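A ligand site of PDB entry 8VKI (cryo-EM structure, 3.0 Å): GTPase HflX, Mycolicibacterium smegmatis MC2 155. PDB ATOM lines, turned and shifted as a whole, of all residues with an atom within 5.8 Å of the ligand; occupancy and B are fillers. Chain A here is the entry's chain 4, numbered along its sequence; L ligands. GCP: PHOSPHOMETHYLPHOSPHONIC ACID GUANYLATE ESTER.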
ATOM      1  N   TYR A 253      -0.279   5.636   7.642  1.00  0.00           N
ATOM      2  CA  TYR A 253       0.427   4.766   6.715  1.00  0.00           C
ATOM      3  C   TYR A 253       1.893   4.664   7.097  1.00  0.00           C
ATOM      4  O   TYR A 253       2.465   5.577   7.708  1.00  0.00           O
ATOM      5  CB  TYR A 253       0.314   5.304   5.291  1.00  0.00           C
ATOM      6  CG  TYR A 253      -0.015   4.233   4.297  1.00  0.00           C
ATOM      7  CD1 TYR A 253      -1.286   3.701   4.204  1.00  0.00           C
ATOM      8  CD2 TYR A 253       0.977   3.703   3.479  1.00  0.00           C
ATOM      9  CE1 TYR A 253      -1.576   2.700   3.309  1.00  0.00           C
ATOM     10  CE2 TYR A 253       0.700   2.707   2.581  1.00  0.00           C
ATOM     11  CZ  TYR A 253      -0.573   2.213   2.503  1.00  0.00           C
ATOM     12  OH  TYR A 253      -0.844   1.214   1.597  1.00  0.00           O
ATOM     13  N   THR A 254       2.510   3.551   6.744  1.00  0.00           N
ATOM     14  CA  THR A 254       3.918   3.368   7.027  1.00  0.00           C
ATOM     15  C   THR A 254       4.757   4.361   6.240  1.00  0.00           C
ATOM     16  O   THR A 254       4.298   4.952   5.260  1.00  0.00           O
ATOM     17  CB  THR A 254       4.345   1.957   6.694  1.00  0.00           C
ATOM     18  OG1 THR A 254       5.747   1.811   6.976  1.00  0.00           O
ATOM     19  CG2 THR A 254       4.108   1.697   5.236  1.00  0.00           C
ATOM     20  N   ASN A 255       5.979   4.584   6.701  1.00  0.00           N
ATOM     21  CA  ASN A 255       6.926   5.524   6.106  1.00  0.00           C
ATOM     22  C   ASN A 255       6.386   6.944   6.049  1.00  0.00           C
ATOM     23  O   ASN A 255       6.910   7.773   5.311  1.00  0.00           O
ATOM     24  CB  ASN A 255       7.352   5.072   4.706  1.00  0.00           C
ATOM     25  CG  ASN A 255       8.619   4.246   4.721  1.00  0.00           C
ATOM     26  OD1 ASN A 255       8.591   3.045   4.470  1.00  0.00           O
ATOM     27  ND2 ASN A 255       9.740   4.893   5.018  1.00  0.00           N
ATOM     28  N   ALA A 256       5.341   7.239   6.814  1.00  0.00           N
ATOM     29  CA  ALA A 256       4.792   8.585   6.920  1.00  0.00           C
ATOM     30  C   ALA A 256       5.337   9.347   8.107  1.00  0.00           C
ATOM     31  O   ALA A 256       4.609  10.146   8.707  1.00  0.00           O
ATOM     32  CB  ALA A 256       3.266   8.546   6.972  1.00  0.00           C
ATOM     33  N   GLY A 257       6.585   9.093   8.487  1.00  0.00           N
ATOM     34  CA  GLY A 257       7.157   9.765   9.628  1.00  0.00           C
ATOM     35  C   GLY A 257       6.467   9.421  10.937  1.00  0.00           C
ATOM     36  O   GLY A 257       6.357  10.292  11.810  1.00  0.00           O
ATOM     37  N   LYS A 258       6.005   8.188  11.086  1.00  0.00           N
ATOM     38  CA  LYS A 258       5.262   7.834  12.295  1.00  0.00           C
ATOM     39  C   LYS A 258       6.190   7.730  13.497  1.00  0.00           C
ATOM     40  O   LYS A 258       5.778   8.067  14.612  1.00  0.00           O
ATOM     41  CB  LYS A 258       4.500   6.539  12.096  1.00  0.00           C
ATOM     42  CG  LYS A 258       3.166   6.706  11.416  1.00  0.00           C
ATOM     43  CD  LYS A 258       2.202   5.618  11.830  1.00  0.00           C
ATOM     44  CE  LYS A 258       2.848   4.245  11.764  1.00  0.00           C
ATOM     45  NZ  LYS A 258       3.302   3.851  10.400  1.00  0.00           N
ATOM     46  N   SER A 259       7.414   7.276  13.291  1.00  0.00           N
ATOM     47  CA  SER A 259       8.385   7.202  14.374  1.00  0.00           C
ATOM     48  C   SER A 259       9.254   8.453  14.475  1.00  0.00           C
ATOM     49  O   SER A 259       9.733   8.780  15.557  1.00  0.00           O
ATOM     50  CB  SER A 259       9.287   5.982  14.195  1.00  0.00           C
ATOM     51  OG  SER A 259       8.511   4.794  14.146  1.00  0.00           O
ATOM     52  N   SER A 260       9.461   9.162  13.362  1.00  0.00           N
ATOM     53  CA  SER A 260      10.195  10.404  13.440  1.00  0.00           C
ATOM     54  C   SER A 260       9.440  11.443  14.265  1.00  0.00           C
ATOM     55  O   SER A 260      10.069  12.228  14.974  1.00  0.00           O
ATOM     56  CB  SER A 260      10.457  10.947  12.036  1.00  0.00           C
ATOM     57  OG  SER A 260       9.223  11.232  11.402  1.00  0.00           O
ATOM     58  N   LEU A 261       8.120  11.448  14.189  1.00  0.00           N
ATOM     59  CA  LEU A 261       7.343  12.363  15.028  1.00  0.00           C
ATOM     60  C   LEU A 261       7.569  12.064  16.502  1.00  0.00           C
ATOM     61  O   LEU A 261       7.715  12.979  17.319  1.00  0.00           O
ATOM     62  CB  LEU A 261       5.866  12.261  14.676  1.00  0.00           C
ATOM     63  CG  LEU A 261       5.077  13.570  14.727  1.00  0.00           C
ATOM     64  CD1 LEU A 261       5.714  14.605  13.816  1.00  0.00           C
ATOM     65  CD2 LEU A 261       3.622  13.359  14.342  1.00  0.00           C
ATOM     66  N   LEU A 271      13.943   3.496  16.338  1.00  0.00           N
ATOM     67  CA  LEU A 271      14.532   3.258  15.026  1.00  0.00           C
ATOM     68  C   LEU A 271      13.702   3.951  13.946  1.00  0.00           C
ATOM     69  O   LEU A 271      12.473   3.893  13.955  1.00  0.00           O
ATOM     70  CB  LEU A 271      14.640   1.763  14.743  1.00  0.00           C
ATOM     71  CG  LEU A 271      13.373   0.938  14.499  1.00  0.00           C
ATOM     72  CD1 LEU A 271      13.648  -0.194  13.543  1.00  0.00           C
ATOM     73  CD2 LEU A 271      12.834   0.388  15.807  1.00  0.00           C
ATOM     74  N   VAL A 272      14.385   4.616  13.023  1.00  0.00           N
ATOM     75  CA  VAL A 272      13.736   5.438  12.016  1.00  0.00           C
ATOM     76  C   VAL A 272      14.131   5.005  10.610  1.00  0.00           C
ATOM     77  O   VAL A 272      14.231   5.843   9.707  1.00  0.00           O
ATOM     78  CB  VAL A 272      14.084   6.919  12.219  1.00  0.00           C
ATOM     79  CG1 VAL A 272      13.279   7.492  13.370  1.00  0.00           C
ATOM     80  CG2 VAL A 272      15.562   7.069  12.490  1.00  0.00           C
ATOM     81  N   GLU A 273      14.343   3.699  10.424  1.00  0.00           N
ATOM     82  CA  GLU A 273      14.794   3.190   9.130  1.00  0.00           C
ATOM     83  C   GLU A 273      13.866   3.627   8.003  1.00  0.00           C
ATOM     84  O   GLU A 273      12.672   3.836   8.191  1.00  0.00           O
ATOM     85  CB  GLU A 273      14.885   1.671   9.167  1.00  0.00           C
ATOM     86  CG  GLU A 273      15.187   1.087  10.539  1.00  0.00           C
ATOM     87  CD  GLU A 273      15.898  -0.254  10.467  1.00  0.00           C
ATOM     88  OE1 GLU A 273      16.130  -0.870  11.525  1.00  0.00           O
ATOM     89  OE2 GLU A 273      16.243  -0.689   9.346  1.00  0.00           O
ATOM     90  N   ASN A 274      14.453   3.787   6.815  1.00  0.00           N
ATOM     91  CA  ASN A 274      13.766   4.292   5.639  1.00  0.00           C
ATOM     92  C   ASN A 274      12.798   3.264   5.074  1.00  0.00           C
ATOM     93  O   ASN A 274      11.758   3.649   4.518  1.00  0.00           O
ATOM     94  CB  ASN A 274      14.828   4.729   4.611  1.00  0.00           C
ATOM     95  CG  ASN A 274      14.266   5.164   3.251  1.00  0.00           C
ATOM     96  OD1 ASN A 274      13.107   4.959   2.911  1.00  0.00           O
ATOM     97  ND2 ASN A 274      15.130   5.785   2.463  1.00  0.00           N
ATOM     98  N   ALA A 275      13.064   1.979   5.273  1.00  0.00           N
ATOM     99  CA  ALA A 275      12.291   0.912   4.661  1.00  0.00           C
ATOM    100  C   ALA A 275      10.871   0.874   5.247  1.00  0.00           C
ATOM    101  O   ALA A 275      10.502   1.665   6.115  1.00  0.00           O
ATOM    102  CB  ALA A 275      13.004  -0.421   4.850  1.00  0.00           C
ATOM    103  N   LEU A 276      10.081  -0.092   4.798  1.00  0.00           N
ATOM    104  CA  LEU A 276       8.712  -0.272   5.235  1.00  0.00           C
ATOM    105  C   LEU A 276       8.727  -0.915   6.612  1.00  0.00           C
ATOM    106  O   LEU A 276       9.750  -0.929   7.286  1.00  0.00           O
ATOM    107  CB  LEU A 276       7.930  -1.088   4.219  1.00  0.00           C
ATOM    108  CG  LEU A 276       6.931  -0.262   3.417  1.00  0.00           C
ATOM    109  CD1 LEU A 276       7.662   0.745   2.528  1.00  0.00           C
ATOM    110  CD2 LEU A 276       6.063  -1.180   2.583  1.00  0.00           C
ATOM    111  N   PHE A 277       7.580  -1.466   7.033  1.00  0.00           N
ATOM    112  CA  PHE A 277       7.279  -1.676   8.449  1.00  0.00           C
ATOM    113  C   PHE A 277       8.479  -2.178   9.222  1.00  0.00           C
ATOM    114  O   PHE A 277       8.952  -3.300   9.015  1.00  0.00           O
ATOM    115  CB  PHE A 277       6.148  -2.684   8.623  1.00  0.00           C
ATOM    116  CG  PHE A 277       5.144  -2.687   7.518  1.00  0.00           C
ATOM    117  CD1 PHE A 277       4.398  -1.560   7.246  1.00  0.00           C
ATOM    118  CD2 PHE A 277       4.951  -3.819   6.759  1.00  0.00           C
ATOM    119  CE1 PHE A 277       3.471  -1.566   6.224  1.00  0.00           C
ATOM    120  CE2 PHE A 277       4.028  -3.832   5.743  1.00  0.00           C
ATOM    121  CZ  PHE A 277       3.283  -2.705   5.471  1.00  0.00           C
ATOM    122  N   ALA A 278       8.987  -1.338  10.109  1.00  0.00           N
ATOM    123  CA  ALA A 278      10.125  -1.676  10.960  1.00  0.00           C
ATOM    124  C   ALA A 278       9.779  -1.525  12.430  1.00  0.00           C
ATOM    125  O   ALA A 278      10.178  -2.371  13.248  1.00  0.00           O
ATOM    126  CB  ALA A 278      11.326  -0.794  10.608  1.00  0.00           C
ATOM    127  N   THR A 279       9.037  -0.492  12.789  1.00  0.00           N
ATOM    128  CA  THR A 279       8.518  -0.376  14.142  1.00  0.00           C
ATOM    129  C   THR A 279       7.314  -1.285  14.264  1.00  0.00           C
ATOM    130  O   THR A 279       6.172  -0.822  14.349  1.00  0.00           O
ATOM    131  CB  THR A 279       8.180   1.075  14.463  1.00  0.00           C
ATOM    132  OG1 THR A 279       9.240   1.920  14.022  1.00  0.00           O
ATOM    133  CG2 THR A 279       8.028   1.239  15.954  1.00  0.00           C
ATOM    134  N   THR A 300       2.468   3.362  16.508  1.00  0.00           N
ATOM    135  CA  THR A 300       1.944   2.057  16.142  1.00  0.00           C
ATOM    136  C   THR A 300       2.796   1.418  15.050  1.00  0.00           C
ATOM    137  O   THR A 300       3.925   1.832  14.787  1.00  0.00           O
ATOM    138  CB  THR A 300       0.482   2.200  15.737  1.00  0.00           C
ATOM    139  OG1 THR A 300       0.397   2.484  14.339  1.00  0.00           O
ATOM    140  CG2 THR A 300      -0.196   3.275  16.553  1.00  0.00           C
ATOM    141  N   VAL A 301       2.247   0.388  14.395  1.00  0.00           N
ATOM    142  CA  VAL A 301       2.985  -0.458  13.476  1.00  0.00           C
ATOM    143  C   VAL A 301       2.976   0.131  12.078  1.00  0.00           C
ATOM    144  O   VAL A 301       4.030   0.450  11.512  1.00  0.00           O
ATOM    145  CB  VAL A 301       2.407  -1.883  13.477  1.00  0.00           C
ATOM    146  CG1 VAL A 301       3.244  -2.785  12.593  1.00  0.00           C
ATOM    147  CG2 VAL A 301       2.346  -2.424  14.882  1.00  0.00           C
ATOM    148  N   GLY A 302       1.789   0.264  11.498  1.00  0.00           N
ATOM    149  CA  GLY A 302       1.690   0.765  10.139  1.00  0.00           C
ATOM    150  C   GLY A 302       0.585   0.109   9.351  1.00  0.00           C
ATOM    151  O   GLY A 302       0.391  -1.110   9.449  1.00  0.00           O
ATOM    152  N   ASN A 369       3.072  15.635   7.007  1.00  0.00           N
ATOM    153  CA  ASN A 369       4.472  15.454   7.352  1.00  0.00           C
ATOM    154  C   ASN A 369       5.276  15.405   6.059  1.00  0.00           C
ATOM    155  O   ASN A 369       4.728  15.106   4.990  1.00  0.00           O
ATOM    156  CB  ASN A 369       4.601  14.178   8.235  1.00  0.00           C
ATOM    157  CG  ASN A 369       6.023  13.666   8.386  1.00  0.00           C
ATOM    158  OD1 ASN A 369       6.838  13.720   7.487  1.00  0.00           O
ATOM    159  ND2 ASN A 369       6.304  13.137   9.575  1.00  0.00           N
ATOM    160  N   LYS A 370       6.569  15.711   6.164  1.00  0.00           N
ATOM    161  CA  LYS A 370       7.465  15.873   5.006  1.00  0.00           C
ATOM    162  C   LYS A 370       7.022  16.994   4.076  1.00  0.00           C
ATOM    163  O   LYS A 370       7.242  16.931   2.866  1.00  0.00           O
ATOM    164  CB  LYS A 370       7.613  14.577   4.199  1.00  0.00           C
ATOM    165  CG  LYS A 370       8.088  13.364   4.950  1.00  0.00           C
ATOM    166  CD  LYS A 370       8.736  12.335   4.054  1.00  0.00           C
ATOM    167  CE  LYS A 370       8.843  11.016   4.791  1.00  0.00           C
ATOM    168  NZ  LYS A 370       9.411   9.927   3.949  1.00  0.00           N
ATOM    169  N   ILE A 371       6.419  18.054   4.620  1.00  0.00           N
ATOM    170  CA  ILE A 371       6.112  19.215   3.787  1.00  0.00           C
ATOM    171  C   ILE A 371       7.340  20.063   3.497  1.00  0.00           C
ATOM    172  O   ILE A 371       7.264  20.985   2.688  1.00  0.00           O
ATOM    173  CB  ILE A 371       4.999  20.088   4.404  1.00  0.00           C
ATOM    174  CG1 ILE A 371       5.161  20.260   5.928  1.00  0.00           C
ATOM    175  CG2 ILE A 371       3.639  19.508   4.080  1.00  0.00           C
ATOM    176  CD1 ILE A 371       6.336  21.116   6.369  1.00  0.00           C
ATOM    177  N   ASP A 372       8.464  19.768   4.146  1.00  0.00           N
ATOM    178  CA  ASP A 372       9.707  20.453   3.830  1.00  0.00           C
ATOM    179  C   ASP A 372      10.192  20.113   2.425  1.00  0.00           C
ATOM    180  O   ASP A 372      10.663  20.997   1.707  1.00  0.00           O
ATOM    181  CB  ASP A 372      10.776  20.089   4.859  1.00  0.00           C
ATOM    182  CG  ASP A 372      10.898  18.605   5.065  1.00  0.00           C
ATOM    183  OD1 ASP A 372      10.237  17.844   4.320  1.00  0.00           O
ATOM    184  OD2 ASP A 372      11.640  18.190   5.978  1.00  0.00           O
ATOM    185  N   ALA A 373      10.090  18.843   2.030  1.00  0.00           N
ATOM    186  CA  ALA A 373      10.502  18.403   0.709  1.00  0.00           C
ATOM    187  C   ALA A 373       9.352  18.387  -0.290  1.00  0.00           C
ATOM    188  O   ALA A 373       9.586  18.129  -1.476  1.00  0.00           O
ATOM    189  CB  ALA A 373      11.137  17.012   0.789  1.00  0.00           C
ATOM    190  N   VAL A 392       3.634  19.617   9.771  1.00  0.00           N
ATOM    191  CA  VAL A 392       4.895  19.449  10.468  1.00  0.00           C
ATOM    192  C   VAL A 392       5.949  18.907   9.517  1.00  0.00           C
ATOM    193  O   VAL A 392       5.645  18.257   8.515  1.00  0.00           O
ATOM    194  CB  VAL A 392       4.716  18.524  11.692  1.00  0.00           C
ATOM    195  CG1 VAL A 392       5.926  18.593  12.607  1.00  0.00           C
ATOM    196  CG2 VAL A 392       3.472  18.887  12.438  1.00  0.00           C
ATOM    197  N   SER A 393       7.214  19.171   9.841  1.00  0.00           N
ATOM    198  CA  SER A 393       8.349  18.632   9.086  1.00  0.00           C
ATOM    199  C   SER A 393       9.279  17.941  10.078  1.00  0.00           C
ATOM    200  O   SER A 393      10.150  18.583  10.659  1.00  0.00           O
ATOM    201  CB  SER A 393       9.072  19.727   8.317  1.00  0.00           C
ATOM    202  OG  SER A 393      10.427  19.385   8.090  1.00  0.00           O
ATOM    203  N   ALA A 394       9.084  16.630  10.254  1.00  0.00           N
ATOM    204  CA  ALA A 394       9.866  15.908  11.259  1.00  0.00           C
ATOM    205  C   ALA A 394      11.356  15.944  10.942  1.00  0.00           C
ATOM    206  O   ALA A 394      12.181  15.918  11.852  1.00  0.00           O
ATOM    207  CB  ALA A 394       9.373  14.482  11.376  1.00  0.00           C
ATOM    208  N   ARG A 395      11.713  15.987   9.661  1.00  0.00           N
ATOM    209  CA  ARG A 395      13.128  16.022   9.290  1.00  0.00           C
ATOM    210  C   ARG A 395      13.790  17.306   9.745  1.00  0.00           C
ATOM    211  O   ARG A 395      15.006  17.341   9.949  1.00  0.00           O
ATOM    212  CB  ARG A 395      13.294  15.855   7.786  1.00  0.00           C
ATOM    213  CG  ARG A 395      14.504  15.041   7.391  1.00  0.00           C
ATOM    214  CD  ARG A 395      14.337  13.583   7.769  1.00  0.00           C
ATOM    215  NE  ARG A 395      15.447  12.769   7.284  1.00  0.00           N
ATOM    216  CZ  ARG A 395      15.514  12.213   6.082  1.00  0.00           C
ATOM    217  NH1 ARG A 395      14.545  12.360   5.201  1.00  0.00           N
ATOM    218  NH2 ARG A 395      16.581  11.491   5.767  1.00  0.00           N
ATOM    219  N   THR A 396      13.015  18.372   9.901  1.00  0.00           N
ATOM    220  CA  THR A 396      13.543  19.665  10.302  1.00  0.00           C
ATOM    221  C   THR A 396      12.936  20.213  11.582  1.00  0.00           C
ATOM    222  O   THR A 396      13.453  21.197  12.111  1.00  0.00           O
ATOM    223  CB  THR A 396      13.354  20.700   9.184  1.00  0.00           C
ATOM    224  OG1 THR A 396      11.955  20.825   8.909  1.00  0.00           O
ATOM    225  CG2 THR A 396      14.072  20.264   7.917  1.00  0.00           C
HETATM  226  PG  GCP L   1       7.180   2.941  10.259  1.00  0.00           P
HETATM  227  O1G GCP L   1       5.709   3.026  10.218  1.00  0.00           O
HETATM  228  O2G GCP L   1       7.675   1.463   9.879  1.00  0.00           O
HETATM  229  O3G GCP L   1       7.720   3.331  11.720  1.00  0.00           O
HETATM  230  C3B GCP L   1       7.835   4.105   9.055  1.00  0.00           C
HETATM  231  PB  GCP L   1       7.411   5.732   9.704  1.00  0.00           P
HETATM  232  O1B GCP L   1       6.104   6.190   9.203  1.00  0.00           O
HETATM  233  O2B GCP L   1       7.372   5.658  11.305  1.00  0.00           O
HETATM  234  O3A GCP L   1       8.555   6.768   9.288  1.00  0.00           O
HETATM  235  PA  GCP L   1       9.871   6.744  10.186  1.00  0.00           P
HETATM  236  O1A GCP L   1       9.924   8.025  10.972  1.00  0.00           O
HETATM  237  O2A GCP L   1       9.934   5.415  10.887  1.00  0.00           O
HETATM  238  O5' GCP L   1      11.007   6.774   9.060  1.00  0.00           O
HETATM  239  C5' GCP L   1      10.630   6.750   7.687  1.00  0.00           C
HETATM  240  C4' GCP L   1      11.313   7.909   6.976  1.00  0.00           C
HETATM  241  O4' GCP L   1      10.506   9.077   6.911  1.00  0.00           O
HETATM  242  C3' GCP L   1      12.587   8.313   7.708  1.00  0.00           C
HETATM  243  O3' GCP L   1      13.723   7.878   6.981  1.00  0.00           O
HETATM  244  C2' GCP L   1      12.544   9.815   7.774  1.00  0.00           C
HETATM  245  O2' GCP L   1      13.763  10.371   7.307  1.00  0.00           O
HETATM  246  C1' GCP L   1      11.391  10.192   6.858  1.00  0.00           C
HETATM  247  N9  GCP L   1      10.743  11.450   7.296  1.00  0.00           N
HETATM  248  C8  GCP L   1       9.847  11.593   8.276  1.00  0.00           C
HETATM  249  N7  GCP L   1       9.459  12.893   8.402  1.00  0.00           N
HETATM  250  C5  GCP L   1      10.119  13.589   7.464  1.00  0.00           C
HETATM  251  C6  GCP L   1      10.170  15.010   7.033  1.00  0.00           C
HETATM  252  O6  GCP L   1       9.496  15.889   7.590  1.00  0.00           O
HETATM  253  N1  GCP L   1      10.987  15.316   6.013  1.00  0.00           N
HETATM  254  C2  GCP L   1      11.741  14.400   5.387  1.00  0.00           C
HETATM  255  N2  GCP L   1      12.536  14.798   4.376  1.00  0.00           N
HETATM  256  N3  GCP L   1      11.730  13.085   5.729  1.00  0.00           N
HETATM  257  C4  GCP L   1      10.956  12.634   6.745  1.00  0.00           C
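NZ of Lys 258 sits at hydrogen-bond distance from O of Tyr 253, 3.3 Å away.
N of Thr 396 sits at hydrogen-bond distance from OG of Ser 393, 3.3 Å away.
OD2 of Asp 372 lies within hydrogen-bond range of OG of Ser 393, at 2.7 Å.
OG of Ser 259 lies within hydrogen-bond range of OG1 of Thr 279 (3.0 Å).
N of Leu 276 lies close to OD1 of Asn 255, at 3.5 Å.
The side-chain amide nitrogen of Asn 255 sits at hydrogen-bond distance from the backbone carbonyl oxygen of Asn 274, 2.4 Å away.
OG of Ser 260 sits at hydrogen-bond distance from O of Gly 257, 3.0 Å away.
O of Ala 275 lies close to OD1 of Asn 255, 2.9 Å away.
An oxygen (O5') of the ligand lies close to the backbone carbonyl oxygen of Glu 273 (3.5 Å).
O of Val 301 sits close to O1G of the ligand, 3.3 Å away.
Merely in contact with the ligand: Ser 393 (3.2 Å), Phe 277 (3.5 Å), Asn 274 (3.8 Å) and Tyr 253 (3.98 Å).
Hydrophobic or aromatic side chains that line the ligand: Ala 394.
The nearest printed residue that does not touch the ligand is Leu 276 (4.1 Å).
O6 of the ligand is in hydrogen-bond range of N of Ala 394, at 2.8 Å.
N of Asn 255 sits at hydrogen-bond distance from O1B of the ligand (3.0 Å).
An oxygen (O1B) of the ligand lies within hydrogen-bond range of the backbone NH (N) of Ala 256.
The backbone NH (N) of Ala 278 is in hydrogen-bond range of an oxygen (O2G) of the ligand, at 3.1 Å.
The side-chain amino group of Lys 258 is in salt-bridge range of an oxygen (O1G) of the ligand (2.6 Å).
An oxygen (O1A) of the ligand lies close to the side-chain hydroxyl (OG) of Ser 260, at 3.3 Å.
O2' of the ligand lies close to NE of Arg 395, at 2.9 Å.
The backbone NH (N) of Lys 258 lies within hydrogen-bond range of an oxygen (O1B) of the ligand, at 2.7 Å.
The backbone NH of Ser 259 lies within hydrogen-bond range of an oxygen (O2B) of the ligand, 2.6 Å away.
O6 of the ligand sits at hydrogen-bond distance from N of Lys 370 (3.3 Å).
The backbone carbonyl oxygen of Val 272 sits at hydrogen-bond distance from an oxygen (O3') of the ligand (3.4 Å).
The side-chain hydroxyl (OG) of Ser 259 lies within hydrogen-bond range of an oxygen (O3G) of the ligand.
The backbone NH of Ser 260 is in hydrogen-bond range of an oxygen (O1A) of the ligand, 2.7 Å away.
OG1 of Thr 254 is in hydrogen-bond range of O1G of the ligand (3.5 Å).
N of Arg 395 is in hydrogen-bond range of O6 of the ligand (3.0 Å).
OD1 of Asn 369 lies close to N7 of the ligand (2.9 Å).
The backbone NH of Gly 257 is in hydrogen-bond range of an oxygen (O1B) of the ligand, at 3.0 Å.
An oxygen (O4') of the ligand sits at hydrogen-bond distance from the side-chain amino group (NZ) of Lys 370, at 3.3 Å.
OD2 of Asp 372 is in hydrogen-bond range of N1 of the ligand (2.9 Å).
OG1 of Thr 279 lies within hydrogen-bond range of O3G of the ligand (3.1 Å).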
